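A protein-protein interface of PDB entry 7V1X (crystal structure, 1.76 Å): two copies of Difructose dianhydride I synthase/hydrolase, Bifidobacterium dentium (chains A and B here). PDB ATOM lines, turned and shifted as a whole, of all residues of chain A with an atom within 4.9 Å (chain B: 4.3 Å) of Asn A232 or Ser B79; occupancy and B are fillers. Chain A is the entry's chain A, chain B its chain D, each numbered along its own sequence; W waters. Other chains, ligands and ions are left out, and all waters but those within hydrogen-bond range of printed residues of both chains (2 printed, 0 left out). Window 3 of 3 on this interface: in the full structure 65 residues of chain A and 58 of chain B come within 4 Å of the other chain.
The side-chain amide nitrogen (ND2) of Asn A232 is in hydrogen-bond range of the side-chain hydroxyl (OG) of Ser B79 (3.2 Å). The side-chain amide nitrogen (ND2) of Asn A231 is in hydrogen-bond range of the backbone carbonyl oxygen (O) of Ala B80, at 3.4 Å. The side-chain amide nitrogen (ND2) of Asn A231 is in hydrogen-bond range of the backbone carbonyl oxygen (O) of Ser B79 (2.8 Å).
No position is printed for both chains. Of the 10 pairs that touch across the chains among the printed residues, none has its exchanged pair printed and touching as well.
Of chain B, only Lys B30 and Ser B79 come within 4 Å of Asn A232. Of chain A, only Pro A228, Asn A231 and Asn A232 come within 4 Å of Ser B79. Printed residues of chain B within 4 Å of Val A233: Lys B30 (3.7 Å). Of the printed residues of chain A, Ala B80 touches Asn A226 (3.2 Å) and Asn A231 (3.4 Å). Printed residues of chain B within 4 Å of Asn A231: Lys B30, Ser B79 and Ala B80. Printed residues of chain B within 4 Å of Pro A228: Leu B76 (3.5 Å) and Ser B79 (3.7 Å). The nearest printed residue of chain B that does not touch Asn A232 is Leu B76 (6.4 Å). The nearest residue of chain A that does not touch Ser B79 is Ser A227 (4.2 Å). The nearest printed residue of chain A that does not touch Ala B80 is Pro A228 (4.4 Å).
ND2 of Asn A232 sits at hydrogen-bond distance from O of Pro A228 (2.9 Å). The side-chain amide oxygen (OD1) of Asn A226 lies close to the side-chain amide oxygen (OD1) of Asn A231.
Water W1 bridges OD1 of Asn A232 (2.6 Å) and OG of Ser B79 (3.2 Å). Water W2 bridges OD1 of Asn A232 (2.7 Å) and NZ of Lys B30 (2.8 Å).
Of the 7 printed residues of chain B, 4 touch a printed residue of chain A. Hydrophobic or aromatic side chains of chain B within 4 Å of the printed part of chain A: Ala B80. Along chain B the printed residues that touch a printed residue of chain A span positions 30 to 80. Among the printed residues, 10 pairs touch across the chains.
Among the printed residues, pairs that only touch across the chains: Asn A226 with Ala B80 (3.2 Å), Asn A231 with Lys B30 (3.3 Å), Asn A232 with Lys B30 (3.4 Å), Pro A228 with Leu B76 (3.5 Å), Val A233 with Lys B30 (3.7 Å), Pro A228 with Ser B79 (3.7 Å) and Thr A234 with Lys B30 (3.7 Å).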
ATOM      1  N   ASN A 226     -29.478 -25.578 -31.899  1.00  0.00           N
ATOM      2  CA  ASN A 226     -28.306 -24.684 -31.837  1.00  0.00           C
ATOM      3  C   ASN A 226     -28.619 -23.395 -32.601  1.00  0.00           C
ATOM      4  O   ASN A 226     -27.685 -22.641 -32.816  1.00  0.00           O
ATOM      5  CB  ASN A 226     -27.019 -25.357 -32.326  1.00  0.00           C
ATOM      6  CG  ASN A 226     -26.480 -26.300 -31.281  1.00  0.00           C
ATOM      7  OD1 ASN A 226     -26.680 -26.068 -30.100  1.00  0.00           O
ATOM      8  ND2 ASN A 226     -25.864 -27.395 -31.682  1.00  0.00           N
ATOM      9  N   SER A 227     -29.870 -23.119 -32.943  1.00  0.00           N
ATOM     10  CA  SER A 227     -30.254 -21.750 -33.367  1.00  0.00           C
ATOM     11  C   SER A 227     -30.030 -20.802 -32.177  1.00  0.00           C
ATOM     12  O   SER A 227     -30.050 -21.198 -31.005  1.00  0.00           O
ATOM     13  CB  SER A 227     -31.667 -21.714 -33.897  1.00  0.00           C
ATOM     14  OG  SER A 227     -32.611 -22.089 -32.908  1.00  0.00           O
ATOM     15  N   PRO A 228     -29.679 -19.523 -32.409  1.00  0.00           N
ATOM     16  CA  PRO A 228     -29.481 -18.597 -31.293  1.00  0.00           C
ATOM     17  C   PRO A 228     -30.687 -18.535 -30.347  1.00  0.00           C
ATOM     18  O   PRO A 228     -30.488 -18.322 -29.160  1.00  0.00           O
ATOM     19  CB  PRO A 228     -29.309 -17.257 -32.031  1.00  0.00           C
ATOM     20  CG  PRO A 228     -28.629 -17.643 -33.306  1.00  0.00           C
ATOM     21  CD  PRO A 228     -29.325 -18.930 -33.703  1.00  0.00           C
ATOM     22  N   GLU A 229     -31.899 -18.699 -30.882  1.00  0.00           N
ATOM     23  CA  GLU A 229     -33.154 -18.540 -30.088  1.00  0.00           C
ATOM     24  C   GLU A 229     -33.208 -19.681 -29.083  1.00  0.00           C
ATOM     25  O   GLU A 229     -33.467 -19.454 -27.896  1.00  0.00           O
ATOM     26  CB  GLU A 229     -34.396 -18.545 -30.975  1.00  0.00           C
ATOM     27  CG  GLU A 229     -34.543 -17.296 -31.837  1.00  0.00           C
ATOM     28  CD  GLU A 229     -33.870 -17.304 -33.201  1.00  0.00           C
ATOM     29  OE1 GLU A 229     -33.071 -18.235 -33.500  1.00  0.00           O
ATOM     30  OE2 GLU A 229     -34.121 -16.365 -33.969  1.00  0.00           O
ATOM     31  N   VAL A 230     -32.895 -20.880 -29.544  1.00  0.00           N
ATOM     32  CA  VAL A 230     -32.837 -22.065 -28.650  1.00  0.00           C
ATOM     33  C   VAL A 230     -31.758 -21.847 -27.604  1.00  0.00           C
ATOM     34  O   VAL A 230     -32.036 -22.066 -26.430  1.00  0.00           O
ATOM     35  CB  VAL A 230     -32.597 -23.348 -29.446  1.00  0.00           C
ATOM     36  CG1 VAL A 230     -32.321 -24.524 -28.523  1.00  0.00           C
ATOM     37  CG2 VAL A 230     -33.784 -23.635 -30.335  1.00  0.00           C
ATOM     38  N   ASN A 231     -30.551 -21.470 -28.009  1.00  0.00           N
ATOM     39  CA  ASN A 231     -29.364 -21.520 -27.128  1.00  0.00           C
ATOM     40  C   ASN A 231     -29.452 -20.471 -26.042  1.00  0.00           C
ATOM     41  O   ASN A 231     -28.747 -20.665 -25.049  1.00  0.00           O
ATOM     42  CB  ASN A 231     -28.069 -21.392 -27.892  1.00  0.00           C
ATOM     43  CG  ASN A 231     -27.699 -22.687 -28.584  1.00  0.00           C
ATOM     44  OD1 ASN A 231     -28.194 -23.745 -28.233  1.00  0.00           O
ATOM     45  ND2 ASN A 231     -26.776 -22.610 -29.524  1.00  0.00           N
ATOM     46  N   ASN A 232     -30.317 -19.478 -26.195  1.00  0.00           N
ATOM     47  CA  ASN A 232     -30.413 -18.357 -25.213  1.00  0.00           C
ATOM     48  C   ASN A 232     -31.600 -18.592 -24.258  1.00  0.00           C
ATOM     49  O   ASN A 232     -31.806 -17.774 -23.388  1.00  0.00           O
ATOM     50  CB  ASN A 232     -30.399 -16.998 -25.931  1.00  0.00           C
ATOM     51  CG  ASN A 232     -29.008 -16.672 -26.477  1.00  0.00           C
ATOM     52  OD1 ASN A 232     -28.008 -16.731 -25.769  1.00  0.00           O
ATOM     53  ND2 ASN A 232     -28.906 -16.387 -27.763  1.00  0.00           N
ATOM     54  N   VAL A 233     -32.307 -19.706 -24.359  1.00  0.00           N
ATOM     55  CA  VAL A 233     -33.302 -20.126 -23.325  1.00  0.00           C
ATOM     56  C   VAL A 233     -32.546 -20.691 -22.125  1.00  0.00           C
ATOM     57  O   VAL A 233     -31.548 -21.391 -22.306  1.00  0.00           O
ATOM     58  CB  VAL A 233     -34.342 -21.103 -23.909  1.00  0.00           C
ATOM     59  CG1 VAL A 233     -35.209 -21.754 -22.854  1.00  0.00           C
ATOM     60  CG2 VAL A 233     -35.226 -20.437 -24.941  1.00  0.00           C
ATOM     61  N   THR A 234     -33.007 -20.384 -20.914  1.00  0.00           N
ATOM     62  CA  THR A 234     -32.333 -20.726 -19.648  1.00  0.00           C
ATOM     63  C   THR A 234     -33.021 -21.940 -19.018  1.00  0.00           C
ATOM     64  O   THR A 234     -34.230 -22.093 -19.163  1.00  0.00           O
ATOM     65  CB  THR A 234     -32.321 -19.557 -18.644  1.00  0.00           C
ATOM     66  OG1 THR A 234     -33.649 -19.347 -18.181  1.00  0.00           O
ATOM     67  CG2 THR A 234     -31.797 -18.273 -19.242  1.00  0.00           C
ATOM     68  N   LYS B  30     -27.783 -21.235 -19.967  1.00  0.00           N
ATOM     69  CA  LYS B  30     -27.956 -21.273 -21.442  1.00  0.00           C
ATOM     70  C   LYS B  30     -27.036 -22.381 -21.978  1.00  0.00           C
ATOM     71  O   LYS B  30     -26.637 -23.258 -21.188  1.00  0.00           O
ATOM     72  CB  LYS B  30     -27.695 -19.872 -22.019  1.00  0.00           C
ATOM     73  CG  LYS B  30     -28.714 -18.826 -21.560  1.00  0.00           C
ATOM     74  CD  LYS B  30     -28.434 -17.416 -21.990  1.00  0.00           C
ATOM     75  CE  LYS B  30     -29.383 -16.394 -21.389  1.00  0.00           C
ATOM     76  NZ  LYS B  30     -29.236 -15.120 -22.129  1.00  0.00           N
ATOM     77  N   GLU B  75     -22.643 -11.443 -34.478  1.00  0.00           N
ATOM     78  CA  GLU B  75     -23.326 -11.339 -33.163  1.00  0.00           C
ATOM     79  C   GLU B  75     -24.234 -12.569 -32.988  1.00  0.00           C
ATOM     80  O   GLU B  75     -24.103 -13.248 -31.993  1.00  0.00           O
ATOM     81  CB  GLU B  75     -24.077 -10.009 -33.053  1.00  0.00           C
ATOM     82  CG  GLU B  75     -23.148  -8.783 -33.053  1.00  0.00           C
ATOM     83  CD  GLU B  75     -22.549  -8.350 -34.382  1.00  0.00           C
ATOM     84  OE1 GLU B  75     -23.266  -8.505 -35.422  1.00  0.00           O
ATOM     85  OE2 GLU B  75     -21.349  -7.895 -34.381  1.00  0.00           O
ATOM     86  N   LEU B  76     -25.127 -12.857 -33.926  1.00  0.00           N
ATOM     87  CA  LEU B  76     -25.982 -14.078 -33.858  1.00  0.00           C
ATOM     88  C   LEU B  76     -25.094 -15.321 -33.850  1.00  0.00           C
ATOM     89  O   LEU B  76     -25.423 -16.283 -33.135  1.00  0.00           O
ATOM     90  CB  LEU B  76     -26.933 -14.097 -35.054  1.00  0.00           C
ATOM     91  CG  LEU B  76     -28.060 -13.062 -34.992  1.00  0.00           C
ATOM     92  CD1 LEU B  76     -28.960 -13.169 -36.203  1.00  0.00           C
ATOM     93  CD2 LEU B  76     -28.868 -13.239 -33.724  1.00  0.00           C
ATOM     94  N   ASN B  77     -24.036 -15.339 -34.663  1.00  0.00           N
ATOM     95  CA  ASN B  77     -23.204 -16.557 -34.802  1.00  0.00           C
ATOM     96  C   ASN B  77     -22.610 -16.952 -33.449  1.00  0.00           C
ATOM     97  O   ASN B  77     -22.465 -18.161 -33.191  1.00  0.00           O
ATOM     98  CB  ASN B  77     -22.136 -16.345 -35.858  1.00  0.00           C
ATOM     99  CG  ASN B  77     -21.398 -17.589 -36.260  1.00  0.00           C
ATOM    100  OD1 ASN B  77     -21.676 -18.722 -35.805  1.00  0.00           O
ATOM    101  ND2 ASN B  77     -20.503 -17.353 -37.189  1.00  0.00           N
ATOM    102  N   ALA B  78     -22.328 -15.976 -32.579  1.00  0.00           N
ATOM    103  CA  ALA B  78     -21.749 -16.248 -31.252  1.00  0.00           C
ATOM    104  C   ALA B  78     -22.681 -17.133 -30.413  1.00  0.00           C
ATOM    105  O   ALA B  78     -22.141 -17.844 -29.515  1.00  0.00           O
ATOM    106  CB  ALA B  78     -21.440 -14.968 -30.511  1.00  0.00           C
ATOM    107  N   SER B  79     -23.997 -17.098 -30.656  1.00  0.00           N
ATOM    108  CA  SER B  79     -25.021 -17.855 -29.885  1.00  0.00           C
ATOM    109  C   SER B  79     -25.441 -19.146 -30.577  1.00  0.00           C
ATOM    110  O   SER B  79     -26.239 -19.875 -29.995  1.00  0.00           O
ATOM    111  CB  SER B  79     -26.228 -17.018 -29.593  1.00  0.00           C
ATOM    112  OG  SER B  79     -25.860 -16.072 -28.628  1.00  0.00           O
ATOM    113  N   ALA B  80     -24.943 -19.436 -31.767  1.00  0.00           N
ATOM    114  CA  ALA B  80     -25.196 -20.726 -32.446  1.00  0.00           C
ATOM    115  C   ALA B  80     -24.249 -21.782 -31.872  1.00  0.00           C
ATOM    116  O   ALA B  80     -23.709 -21.587 -30.716  1.00  0.00           O
ATOM    117  CB  ALA B  80     -25.049 -20.554 -33.930  1.00  0.00           C
HETATM  118  O   HOH W   1     -25.712 -15.504 -25.463  1.00  0.00           O
HETATM  119  O   HOH W   2     -27.820 -14.352 -24.425  1.00  0.00           O
